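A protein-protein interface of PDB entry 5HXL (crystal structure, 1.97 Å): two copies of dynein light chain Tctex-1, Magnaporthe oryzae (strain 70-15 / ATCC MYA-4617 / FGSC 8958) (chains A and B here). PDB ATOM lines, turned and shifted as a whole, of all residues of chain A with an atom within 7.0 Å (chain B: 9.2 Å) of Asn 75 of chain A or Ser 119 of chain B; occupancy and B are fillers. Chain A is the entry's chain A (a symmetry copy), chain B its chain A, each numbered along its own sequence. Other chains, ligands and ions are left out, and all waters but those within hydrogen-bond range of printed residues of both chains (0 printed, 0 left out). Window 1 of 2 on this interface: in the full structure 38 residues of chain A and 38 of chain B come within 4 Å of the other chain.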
ATOM      1  N   THR A  40      20.929   6.790 -35.293  1.00  0.00           N
ATOM      2  CA  THR A  40      20.934   7.193 -33.874  1.00  0.00           C
ATOM      3  C   THR A  40      21.863   8.372 -33.608  1.00  0.00           C
ATOM      4  O   THR A  40      21.570   9.220 -32.766  1.00  0.00           O
ATOM      5  CB  THR A  40      21.347   6.027 -32.931  1.00  0.00           C
ATOM      6  OG1 THR A  40      22.564   5.426 -33.395  1.00  0.00           O
ATOM      7  CG2 THR A  40      20.263   4.986 -32.872  1.00  0.00           C
ATOM      8  N   ASN A  44      20.414  11.740 -31.927  1.00  0.00           N
ATOM      9  CA  ASN A  44      20.947  12.254 -30.681  1.00  0.00           C
ATOM     10  C   ASN A  44      21.526  13.665 -30.827  1.00  0.00           C
ATOM     11  O   ASN A  44      21.308  14.524 -29.959  1.00  0.00           O
ATOM     12  CB  ASN A  44      22.032  11.326 -30.131  1.00  0.00           C
ATOM     13  CG  ASN A  44      21.487  10.305 -29.149  1.00  0.00           C
ATOM     14  OD1 ASN A  44      20.451  10.514 -28.530  1.00  0.00           O
ATOM     15  ND2 ASN A  44      22.187   9.190 -29.010  1.00  0.00           N
ATOM     16  N   HIS A  45      22.264  13.895 -31.915  1.00  0.00           N
ATOM     17  CA  HIS A  45      22.852  15.212 -32.183  1.00  0.00           C
ATOM     18  C   HIS A  45      21.792  16.287 -32.298  1.00  0.00           C
ATOM     19  O   HIS A  45      21.948  17.385 -31.755  1.00  0.00           O
ATOM     20  CB  HIS A  45      23.670  15.207 -33.466  1.00  0.00           C
ATOM     21  CG  HIS A  45      24.973  14.493 -33.354  1.00  0.00           C
ATOM     22  ND1 HIS A  45      25.572  14.233 -32.139  1.00  0.00           N
ATOM     23  CD2 HIS A  45      25.809  14.003 -34.297  1.00  0.00           C
ATOM     24  CE1 HIS A  45      26.715  13.611 -32.347  1.00  0.00           C
ATOM     25  NE2 HIS A  45      26.880  13.449 -33.648  1.00  0.00           N
ATOM     26  N   ILE A  47      18.665  16.158 -31.081  1.00  0.00           N
ATOM     27  CA  ILE A  47      18.016  16.332 -29.778  1.00  0.00           C
ATOM     28  C   ILE A  47      18.834  17.230 -28.845  1.00  0.00           C
ATOM     29  O   ILE A  47      18.322  18.183 -28.253  1.00  0.00           O
ATOM     30  CB  ILE A  47      17.784  14.959 -29.104  1.00  0.00           C
ATOM     31  CG1 ILE A  47      16.804  14.123 -29.943  1.00  0.00           C
ATOM     32  CG2 ILE A  47      17.259  15.125 -27.680  1.00  0.00           C
ATOM     33  CD1 ILE A  47      16.660  12.650 -29.475  1.00  0.00           C
ATOM     34  N   ILE A  48      20.118  16.923 -28.722  1.00  0.00           N
ATOM     35  CA  ILE A  48      20.996  17.658 -27.828  1.00  0.00           C
ATOM     36  C   ILE A  48      21.173  19.110 -28.252  1.00  0.00           C
ATOM     37  O   ILE A  48      21.130  20.034 -27.418  1.00  0.00           O
ATOM     38  CB  ILE A  48      22.363  16.978 -27.741  1.00  0.00           C
ATOM     39  CG1 ILE A  48      22.235  15.732 -26.879  1.00  0.00           C
ATOM     40  CG2 ILE A  48      23.404  17.901 -27.124  1.00  0.00           C
ATOM     41  CD1 ILE A  48      23.457  14.910 -26.884  1.00  0.00           C
ATOM     42  N   ILE A  51      17.862  21.001 -27.469  1.00  0.00           N
ATOM     43  CA  ILE A  51      17.687  21.255 -26.040  1.00  0.00           C
ATOM     44  C   ILE A  51      18.688  22.298 -25.550  1.00  0.00           C
ATOM     45  O   ILE A  51      18.303  23.260 -24.890  1.00  0.00           O
ATOM     46  CB  ILE A  51      17.828  19.962 -25.215  1.00  0.00           C
ATOM     47  CG1 ILE A  51      16.697  18.989 -25.579  1.00  0.00           C
ATOM     48  CG2 ILE A  51      17.791  20.268 -23.697  1.00  0.00           C
ATOM     49  CD1 ILE A  51      16.819  17.595 -24.977  1.00  0.00           C
ATOM     50  N   ALA A  73      25.105  20.664 -18.868  1.00  0.00           N
ATOM     51  CA  ALA A  73      25.455  19.491 -19.630  1.00  0.00           C
ATOM     52  C   ALA A  73      24.160  18.762 -19.982  1.00  0.00           C
ATOM     53  O   ALA A  73      23.268  18.635 -19.155  1.00  0.00           O
ATOM     54  CB  ALA A  73      26.394  18.597 -18.859  1.00  0.00           C
ATOM     55  N   VAL A  74      24.070  18.297 -21.221  1.00  0.00           N
ATOM     56  CA  VAL A  74      22.894  17.597 -21.696  1.00  0.00           C
ATOM     57  C   VAL A  74      23.300  16.267 -22.301  1.00  0.00           C
ATOM     58  O   VAL A  74      24.109  16.239 -23.229  1.00  0.00           O
ATOM     59  CB  VAL A  74      22.139  18.411 -22.772  1.00  0.00           C
ATOM     60  CG1 VAL A  74      20.974  17.586 -23.335  1.00  0.00           C
ATOM     61  CG2 VAL A  74      21.646  19.733 -22.206  1.00  0.00           C
ATOM     62  N   ASN A  75      22.738  15.180 -21.782  1.00  0.00           N
ATOM     63  CA  ASN A  75      22.975  13.853 -22.327  1.00  0.00           C
ATOM     64  C   ASN A  75      21.692  13.284 -22.916  1.00  0.00           C
ATOM     65  O   ASN A  75      20.616  13.458 -22.361  1.00  0.00           O
ATOM     66  CB  ASN A  75      23.526  12.913 -21.253  1.00  0.00           C
ATOM     67  CG  ASN A  75      23.733  11.489 -21.777  1.00  0.00           C
ATOM     68  OD1 ASN A  75      22.861  10.632 -21.640  1.00  0.00           O
ATOM     69  ND2 ASN A  75      24.879  11.245 -22.404  1.00  0.00           N
ATOM     70  N   SER A  76      21.810  12.628 -24.065  1.00  0.00           N
ATOM     71  CA  SER A  76      20.668  12.000 -24.691  1.00  0.00           C
ATOM     72  C   SER A  76      21.045  10.573 -25.003  1.00  0.00           C
ATOM     73  O   SER A  76      22.123  10.322 -25.550  1.00  0.00           O
ATOM     74  CB  SER A  76      20.255  12.736 -25.966  1.00  0.00           C
ATOM     75  OG  SER A  76      19.148  12.094 -26.572  1.00  0.00           O
ATOM     76  N   THR A  77      20.170   9.640 -24.643  1.00  0.00           N
ATOM     77  CA  THR A  77      20.413   8.235 -24.944  1.00  0.00           C
ATOM     78  C   THR A  77      19.223   7.623 -25.653  1.00  0.00           C
ATOM     79  O   THR A  77      18.091   7.775 -25.201  1.00  0.00           O
ATOM     80  CB  THR A  77      20.713   7.423 -23.661  1.00  0.00           C
ATOM     81  OG1 THR A  77      21.782   8.047 -22.958  1.00  0.00           O
ATOM     82  CG2 THR A  77      21.122   5.982 -24.007  1.00  0.00           C
ATOM     83  N   ILE A  78      19.486   6.948 -26.768  1.00  0.00           N
ATOM     84  CA  ILE A  78      18.456   6.218 -27.497  1.00  0.00           C
ATOM     85  C   ILE A  78      18.634   4.733 -27.239  1.00  0.00           C
ATOM     86  O   ILE A  78      19.718   4.182 -27.451  1.00  0.00           O
ATOM     87  CB  ILE A  78      18.503   6.515 -29.014  1.00  0.00           C
ATOM     88  CG1 ILE A  78      18.248   8.006 -29.243  1.00  0.00           C
ATOM     89  CG2 ILE A  78      17.482   5.667 -29.755  1.00  0.00           C
ATOM     90  CD1 ILE A  78      18.425   8.441 -30.663  1.00  0.00           C
ATOM     91  N   VAL A 148      15.918   8.710 -23.601  1.00  0.00           N
ATOM     92  CA  VAL A 148      16.094   9.250 -22.266  1.00  0.00           C
ATOM     93  C   VAL A 148      17.013  10.469 -22.320  1.00  0.00           C
ATOM     94  O   VAL A 148      18.088  10.410 -22.911  1.00  0.00           O
ATOM     95  CB  VAL A 148      16.675   8.198 -21.307  1.00  0.00           C
ATOM     96  CG1 VAL A 148      17.044   8.836 -19.989  1.00  0.00           C
ATOM     97  CG2 VAL A 148      15.653   7.097 -21.085  1.00  0.00           C
ATOM     98  N   VAL A 149      16.576  11.563 -21.697  1.00  0.00           N
ATOM     99  CA  VAL A 149      17.315  12.824 -21.692  1.00  0.00           C
ATOM    100  C   VAL A 149      17.650  13.191 -20.242  1.00  0.00           C
ATOM    101  O   VAL A 149      16.834  13.000 -19.343  1.00  0.00           O
ATOM    102  CB  VAL A 149      16.503  13.970 -22.351  1.00  0.00           C
ATOM    103  CG1 VAL A 149      17.148  15.322 -22.083  1.00  0.00           C
ATOM    104  CG2 VAL A 149      16.366  13.741 -23.852  1.00  0.00           C
ATOM    105  N   MET A 150      18.853  13.699 -20.021  1.00  0.00           N
ATOM    106  CA  MET A 150      19.197  14.230 -18.713  1.00  0.00           C
ATOM    107  C   MET A 150      19.928  15.547 -18.864  1.00  0.00           C
ATOM    108  O   MET A 150      20.779  15.722 -19.749  1.00  0.00           O
ATOM    109  CB  MET A 150      20.024  13.237 -17.916  1.00  0.00           C
ATOM    110  CG  MET A 150      21.445  13.091 -18.358  1.00  0.00           C
ATOM    111  SD  MET A 150      22.373  12.234 -17.079  1.00  0.00           S
ATOM    112  CE  MET A 150      22.346  13.487 -15.820  1.00  0.00           C
ATOM    113  N   LEU A 151      19.545  16.490 -18.022  1.00  0.00           N
ATOM    114  CA  LEU A 151      20.112  17.828 -18.027  1.00  0.00           C
ATOM    115  C   LEU A 151      20.679  18.073 -16.638  1.00  0.00           C
ATOM    116  O   LEU A 151      20.013  17.789 -15.643  1.00  0.00           O
ATOM    117  CB  LEU A 151      19.048  18.883 -18.378  1.00  0.00           C
ATOM    118  CG  LEU A 151      19.422  20.330 -17.996  1.00  0.00           C
ATOM    119  CD1 LEU A 151      20.377  20.954 -19.021  1.00  0.00           C
ATOM    120  CD2 LEU A 151      18.198  21.203 -17.793  1.00  0.00           C
ATOM    121  N   ILE A 152      21.918  18.549 -16.584  1.00  0.00           N
ATOM    122  CA  ILE A 152      22.563  18.960 -15.345  1.00  0.00           C
ATOM    123  C   ILE A 152      22.787  20.472 -15.420  1.00  0.00           C
ATOM    124  O   ILE A 152      23.216  20.969 -16.458  1.00  0.00           O
ATOM    125  CB  ILE A 152      23.931  18.250 -15.139  1.00  0.00           C
ATOM    126  CG1 ILE A 152      23.764  16.726 -15.040  1.00  0.00           C
ATOM    127  CG2 ILE A 152      24.669  18.807 -13.916  1.00  0.00           C
ATOM    128  CD1 ILE A 152      23.694  16.209 -13.632  1.00  0.00           C
ATOM    129  N   HIS B   1      29.219   6.040 -26.973  1.00  0.00           N
ATOM    130  CA  HIS B   1      29.056   7.430 -26.551  1.00  0.00           C
ATOM    131  C   HIS B   1      30.123   8.328 -27.137  1.00  0.00           C
ATOM    132  O   HIS B   1      31.254   7.909 -27.358  1.00  0.00           O
ATOM    133  CB  HIS B   1      29.078   7.542 -25.027  1.00  0.00           C
ATOM    134  CG  HIS B   1      28.914   8.943 -24.525  1.00  0.00           C
ATOM    135  ND1 HIS B   1      29.957   9.844 -24.483  1.00  0.00           N
ATOM    136  CD2 HIS B   1      27.826   9.604 -24.061  1.00  0.00           C
ATOM    137  CE1 HIS B   1      29.521  10.997 -24.010  1.00  0.00           C
ATOM    138  NE2 HIS B   1      28.232  10.879 -23.747  1.00  0.00           N
ATOM    139  N   HIS B   2      29.758   9.576 -27.374  1.00  0.00           N
ATOM    140  CA  HIS B   2      30.719  10.561 -27.827  1.00  0.00           C
ATOM    141  C   HIS B   2      30.274  11.965 -27.462  1.00  0.00           C
ATOM    142  O   HIS B   2      29.078  12.288 -27.488  1.00  0.00           O
ATOM    143  CB  HIS B   2      30.889  10.457 -29.320  1.00  0.00           C
ATOM    144  CG  HIS B   2      29.589  10.504 -30.037  1.00  0.00           C
ATOM    145  ND1 HIS B   2      29.025  11.684 -30.466  1.00  0.00           N
ATOM    146  CD2 HIS B   2      28.715   9.525 -30.358  1.00  0.00           C
ATOM    147  CE1 HIS B   2      27.870  11.421 -31.042  1.00  0.00           C
ATOM    148  NE2 HIS B   2      27.660  10.120 -30.996  1.00  0.00           N
ATOM    149  N   SER B   3      31.249  12.793 -27.115  1.00  0.00           N
ATOM    150  CA  SER B   3      30.965  14.149 -26.716  1.00  0.00           C
ATOM    151  C   SER B   3      30.878  15.035 -27.953  1.00  0.00           C
ATOM    152  O   SER B   3      31.650  14.885 -28.907  1.00  0.00           O
ATOM    153  CB  SER B   3      32.038  14.668 -25.747  1.00  0.00           C
ATOM    154  OG  SER B   3      31.543  15.742 -24.955  1.00  0.00           O
ATOM    155  N   MET B   4      29.925  15.950 -27.933  1.00  0.00           N
ATOM    156  CA  MET B   4      29.796  16.950 -28.978  1.00  0.00           C
ATOM    157  C   MET B   4      30.538  18.230 -28.618  1.00  0.00           C
ATOM    158  O   MET B   4      30.676  19.118 -29.452  1.00  0.00           O
ATOM    159  CB  MET B   4      28.329  17.268 -29.224  1.00  0.00           C
ATOM    160  CG  MET B   4      27.461  16.049 -29.458  1.00  0.00           C
ATOM    161  SD  MET B   4      25.737  16.536 -29.430  1.00  0.00           S
ATOM    162  CE  MET B   4      25.666  17.672 -30.800  1.00  0.00           C
ATOM    163  N   ASN B  75      27.156   9.428 -13.053  1.00  0.00           N
ATOM    164  CA  ASN B  75      25.991   8.645 -13.428  1.00  0.00           C
ATOM    165  C   ASN B  75      26.389   7.204 -13.715  1.00  0.00           C
ATOM    166  O   ASN B  75      27.429   6.947 -14.308  1.00  0.00           O
ATOM    167  CB  ASN B  75      25.293   9.253 -14.646  1.00  0.00           C
ATOM    168  CG  ASN B  75      24.093   8.421 -15.107  1.00  0.00           C
ATOM    169  OD1 ASN B  75      24.215   7.570 -15.989  1.00  0.00           O
ATOM    170  ND2 ASN B  75      22.939   8.645 -14.489  1.00  0.00           N
ATOM    171  N   THR B  77      24.689   3.525 -15.184  1.00  0.00           N
ATOM    172  CA  THR B  77      23.537   2.864 -15.785  1.00  0.00           C
ATOM    173  C   THR B  77      23.808   1.388 -15.986  1.00  0.00           C
ATOM    174  O   THR B  77      24.846   1.020 -16.532  1.00  0.00           O
ATOM    175  CB  THR B  77      23.161   3.502 -17.143  1.00  0.00           C
ATOM    176  OG1 THR B  77      22.982   4.903 -16.962  1.00  0.00           O
ATOM    177  CG2 THR B  77      21.854   2.902 -17.688  1.00  0.00           C
ATOM    178  N   GLY B 116      21.613  -2.516 -28.340  1.00  0.00           N
ATOM    179  CA  GLY B 116      21.211  -1.364 -29.127  1.00  0.00           C
ATOM    180  C   GLY B 116      21.093  -0.119 -28.262  1.00  0.00           C
ATOM    181  O   GLY B 116      20.051   0.163 -27.670  1.00  0.00           O
ATOM    182  N   MET B 117      22.174   0.635 -28.175  1.00  0.00           N
ATOM    183  CA  MET B 117      22.178   1.807 -27.320  1.00  0.00           C
ATOM    184  C   MET B 117      23.187   2.835 -27.792  1.00  0.00           C
ATOM    185  O   MET B 117      24.363   2.520 -27.974  1.00  0.00           O
ATOM    186  CB  MET B 117      22.486   1.406 -25.885  1.00  0.00           C
ATOM    187  CG  MET B 117      22.323   2.524 -24.886  1.00  0.00           C
ATOM    188  SD  MET B 117      22.454   1.875 -23.216  1.00  0.00           S
ATOM    189  CE  MET B 117      24.087   1.139 -23.286  1.00  0.00           C
ATOM    190  N   HIS B 118      22.728   4.064 -27.985  1.00  0.00           N
ATOM    191  CA  HIS B 118      23.622   5.125 -28.400  1.00  0.00           C
ATOM    192  C   HIS B 118      23.415   6.358 -27.555  1.00  0.00           C
ATOM    193  O   HIS B 118      22.288   6.792 -27.324  1.00  0.00           O
ATOM    194  CB  HIS B 118      23.433   5.482 -29.876  1.00  0.00           C
ATOM    195  CG  HIS B 118      24.397   6.523 -30.352  1.00  0.00           C
ATOM    196  ND1 HIS B 118      25.618   6.212 -30.911  1.00  0.00           N
ATOM    197  CD2 HIS B 118      24.345   7.876 -30.293  1.00  0.00           C
ATOM    198  CE1 HIS B 118      26.262   7.329 -31.205  1.00  0.00           C
ATOM    199  NE2 HIS B 118      25.512   8.353 -30.834  1.00  0.00           N
ATOM    200  N   SER B 119      24.515   6.926 -27.090  1.00  0.00           N
ATOM    201  CA  SER B 119      24.415   8.051 -26.192  1.00  0.00           C
ATOM    202  C   SER B 119      25.260   9.204 -26.724  1.00  0.00           C
ATOM    203  O   SER B 119      26.249   8.987 -27.432  1.00  0.00           O
ATOM    204  CB  SER B 119      24.853   7.646 -24.780  1.00  0.00           C
ATOM    205  OG  SER B 119      24.648   8.703 -23.863  1.00  0.00           O
ATOM    206  N   ALA B 120      24.856  10.427 -26.404  1.00  0.00           N
ATOM    207  CA  ALA B 120      25.641  11.596 -26.769  1.00  0.00           C
ATOM    208  C   ALA B 120      25.540  12.664 -25.691  1.00  0.00           C
ATOM    209  O   ALA B 120      24.557  12.724 -24.970  1.00  0.00           O
ATOM    210  CB  ALA B 120      25.190  12.151 -28.116  1.00  0.00           C
ATOM    211  N   THR B 121      26.548  13.527 -25.613  1.00  0.00           N
ATOM    212  CA  THR B 121      26.561  14.586 -24.615  1.00  0.00           C
ATOM    213  C   THR B 121      27.022  15.901 -25.235  1.00  0.00           C
ATOM    214  O   THR B 121      27.996  15.937 -25.995  1.00  0.00           O
ATOM    215  CB  THR B 121      27.490  14.243 -23.431  1.00  0.00           C
ATOM    216  OG1 THR B 121      27.029  13.058 -22.770  1.00  0.00           O
ATOM    217  CG2 THR B 121      27.513  15.386 -22.420  1.00  0.00           C
ATOM    218  N   GLY B 122      26.309  16.970 -24.912  1.00  0.00           N
ATOM    219  CA  GLY B 122      26.684  18.309 -25.312  1.00  0.00           C
ATOM    220  C   GLY B 122      26.746  19.169 -24.065  1.00  0.00           C
ATOM    221  O   GLY B 122      26.264  18.774 -23.015  1.00  0.00           O
ATOM    222  N   ALA B 123      27.356  20.346 -24.155  1.00  0.00           N
ATOM    223  CA  ALA B 123      27.486  21.161 -22.953  1.00  0.00           C
ATOM    224  C   ALA B 123      27.627  22.647 -23.238  1.00  0.00           C
ATOM    225  O   ALA B 123      28.037  23.057 -24.314  1.00  0.00           O
ATOM    226  CB  ALA B 123      28.674  20.688 -22.128  1.00  0.00           C
ATOM    227  N   MET B 132      34.155  15.538 -19.462  1.00  0.00           N
ATOM    228  CA  MET B 132      33.484  14.303 -19.136  1.00  0.00           C
ATOM    229  C   MET B 132      34.359  13.132 -19.515  1.00  0.00           C
ATOM    230  O   MET B 132      35.265  13.264 -20.337  1.00  0.00           O
ATOM    231  CB  MET B 132      32.153  14.211 -19.870  1.00  0.00           C
ATOM    232  CG  MET B 132      32.317  14.185 -21.374  1.00  0.00           C
ATOM    233  SD  MET B 132      30.713  14.127 -22.155  1.00  0.00           S
ATOM    234  CE  MET B 132      30.011  12.732 -21.281  1.00  0.00           C
ATOM    235  N   THR B 134      33.817   8.642 -19.905  1.00  0.00           N
ATOM    236  CA  THR B 134      32.853   7.553 -19.858  1.00  0.00           C
ATOM    237  C   THR B 134      33.556   6.213 -19.820  1.00  0.00           C
ATOM    238  O   THR B 134      34.669   6.067 -20.316  1.00  0.00           O
ATOM    239  CB  THR B 134      31.891   7.563 -21.073  1.00  0.00           C
ATOM    240  OG1 THR B 134      32.644   7.378 -22.274  1.00  0.00           O
ATOM    241  CG2 THR B 134      31.140   8.875 -21.160  1.00  0.00           C
ATOM    242  N   LYS B 136      32.736   1.824 -20.046  1.00  0.00           N
ATOM    243  CA  LYS B 136      31.837   0.685 -20.195  1.00  0.00           C
ATOM    244  C   LYS B 136      32.459  -0.553 -19.572  1.00  0.00           C
ATOM    245  O   LYS B 136      33.579  -0.936 -19.905  1.00  0.00           O
ATOM    246  CB  LYS B 136      31.502   0.439 -21.673  1.00  0.00           C
ATOM    247  CG  LYS B 136      30.378  -0.575 -21.893  1.00  0.00           C
ATOM    248  CD  LYS B 136      29.609  -0.289 -23.180  1.00  0.00           C
ATOM    249  CE  LYS B 136      28.376  -1.181 -23.310  1.00  0.00           C
ATOM    250  NZ  LYS B 136      27.479  -0.773 -24.439  1.00  0.00           N
ATOM    251  N   VAL B 148      27.449   1.063 -17.706  1.00  0.00           N
ATOM    252  CA  VAL B 148      28.037   2.259 -18.283  1.00  0.00           C
ATOM    253  C   VAL B 148      28.135   3.351 -17.221  1.00  0.00           C
ATOM    254  O   VAL B 148      27.159   3.635 -16.532  1.00  0.00           O
ATOM    255  CB  VAL B 148      27.215   2.764 -19.481  1.00  0.00           C
ATOM    256  CG1 VAL B 148      27.720   4.113 -19.932  1.00  0.00           C
ATOM    257  CG2 VAL B 148      27.312   1.764 -20.620  1.00  0.00           C
ATOM    258  N   VAL B 149      29.318   3.953 -17.104  1.00  0.00           N
ATOM    259  CA  VAL B 149      29.589   4.988 -16.108  1.00  0.00           C
ATOM    260  C   VAL B 149      29.983   6.278 -16.835  1.00  0.00           C
ATOM    261  O   VAL B 149      30.698   6.241 -17.834  1.00  0.00           O
ATOM    262  CB  VAL B 149      30.719   4.565 -15.133  1.00  0.00           C
ATOM    263  CG1 VAL B 149      31.189   5.747 -14.296  1.00  0.00           C
ATOM    264  CG2 VAL B 149      30.256   3.431 -14.227  1.00  0.00           C
ATOM    265  N   MET B 150      29.501   7.408 -16.341  1.00  0.00           N
ATOM    266  CA  MET B 150      29.954   8.689 -16.859  1.00  0.00           C
ATOM    267  C   MET B 150      30.223   9.645 -15.715  1.00  0.00           C
ATOM    268  O   MET B 150      29.475   9.705 -14.728  1.00  0.00           O
ATOM    269  CB  MET B 150      28.948   9.276 -17.834  1.00  0.00           C
ATOM    270  CG  MET B 150      27.709   9.835 -17.211  1.00  0.00           C
ATOM    271  SD  MET B 150      26.850  10.849 -18.420  1.00  0.00           S
ATOM    272  CE  MET B 150      28.016  12.184 -18.551  1.00  0.00           C
ATOM    273  N   ILE B 152      31.330  13.683 -14.923  1.00  0.00           N
ATOM    274  CA  ILE B 152      31.470  15.058 -15.384  1.00  0.00           C
ATOM    275  C   ILE B 152      32.250  15.826 -14.314  1.00  0.00           C
ATOM    276  O   ILE B 152      31.969  15.666 -13.129  1.00  0.00           O
ATOM    277  CB  ILE B 152      30.092  15.741 -15.601  1.00  0.00           C
ATOM    278  CG1 ILE B 152      29.270  15.019 -16.681  1.00  0.00           C
ATOM    279  CG2 ILE B 152      30.254  17.230 -15.932  1.00  0.00           C
ATOM    280  CD1 ILE B 152      29.383  15.632 -18.047  1.00  0.00           C
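N of Ile 152 of chain A is in hydrogen-bond range of O of Ala 73 of chain A. The side-chain amide oxygen (OD1) of Asn 44 of chain A is in hydrogen-bond range of the side-chain hydroxyl (OG) of Ser 76 of chain A, 2.8 Å away. The side-chain amide oxygen (OD1) of Asn 75 of chain A sits at hydrogen-bond distance from the side-chain hydroxyl (OG1) of Thr 77 of chain A (3.1 Å). NE2 of His 1 of chain B lies within hydrogen-bond range of OG1 of Thr 121 of chain B (2.7 Å). The backbone NH of Asn 75 of chain A sits at hydrogen-bond distance from the backbone carbonyl oxygen of Met 150 of chain A (2.9 Å). O of His 2 of chain B is in hydrogen-bond range of N of Thr 121 of chain B.
Of the 21 printed residues of chain B, 9 touch a printed residue of chain A. Hydrophobic or aromatic side chains of chain B within 4 Å of the printed part of chain A: His 1, His 2, Met 4, Met 117, His 118 and Ala 120. Among the printed residues, no Asp or Glu carboxylate lies within 4 Å of a Lys or Arg side-chain nitrogen of the other chain.
6 positions are printed for both chains.
CA of Ser 119 of chain B touches ND2 of Asn 44 of chain A, 3.8 Å away. Met 4 of chain B touches Ile 48 of chain A (SD to CG2, 3.6 Å). Ile 48 of chain A touches Ala 120 of chain B. N of Thr 121 of chain B touches CD1 of Ile 48 of chain A, 3.6 Å away. CA of Ala 73 of chain A touches O of Gly 122 of chain B, 3.6 Å away. Ala 120 of chain B touches Val 74 of chain A (O to O, 3.9 Å). Asn 75 of chain A touches His 1 of chain B. Thr 77 of chain A touches Met 117 of chain B. His 118 of chain B touches Thr 77 of chain A. Ile 78 of chain A touches Met 117 of chain B.
O of Ser 76 of chain A is in hydrogen-bond range of N of Ala 120 of chain B (2.9 Å). The side-chain sulfur (SD) of Met 4 of chain B is in hydrogen-bond range of a ring nitrogen (ND1) of His 45 of chain A (3.6 Å). The side-chain amide nitrogen of Asn 75 of chain A sits at hydrogen-bond distance from the backbone carbonyl oxygen of Ala 120 of chain B, 3.0 Å away. OG of Ser 119 of chain B lies within hydrogen-bond range of ND2 of Asn 75 of chain A (2.9 Å). The backbone NH (N) of Gly 122 of chain B is in hydrogen-bond range of the backbone carbonyl oxygen (O) of Val 74 of chain A (2.9 Å). The side-chain hydroxyl (OG) of Ser 119 of chain B sits at hydrogen-bond distance from the side-chain hydroxyl (OG1) of Thr 77 of chain A (3.1 Å). The backbone carbonyl oxygen (O) of His 118 of chain B sits close to the side-chain amide nitrogen (ND2) of Asn 44 of chain A (2.9 Å). OG of Ser 119 of chain B lies close to O of Ser 76 of chain A, at 3.4 Å. The backbone carbonyl oxygen of His 118 of chain B sits at hydrogen-bond distance from the backbone NH of Ile 78 of chain A (2.9 Å). The side-chain hydroxyl (OG1) of Thr 121 of chain B sits at hydrogen-bond distance from the side-chain amide nitrogen (ND2) of Asn 75 of chain A.
Ser 119 of chain B touches four residues of chain A. Val 74 of chain A touches three residues of chain B. Of the printed residues of chain A, Ala 120 of chain B touches Asn 44, Ile 48, Val 74, Asn 75 and Ser 76. Of the printed residues of chain B, Ala 73 of chain A touches Gly 122. Of the printed residues of chain A, Thr 121 of chain B touches Ile 48, Val 74 and Asn 75. Printed residues of chain A within 4 Å of Gly 122 of chain B: Ile 48 (3.8 Å), Ala 73 (3.6 Å) and Val 74 (2.9 Å). Printed residues of chain B within 4 Å of Ile 78 of chain A: Met 117 and His 118. The nearest printed residue of chain B that does not touch Asn 44 of chain A is Met 4 of chain B (4.9 Å).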
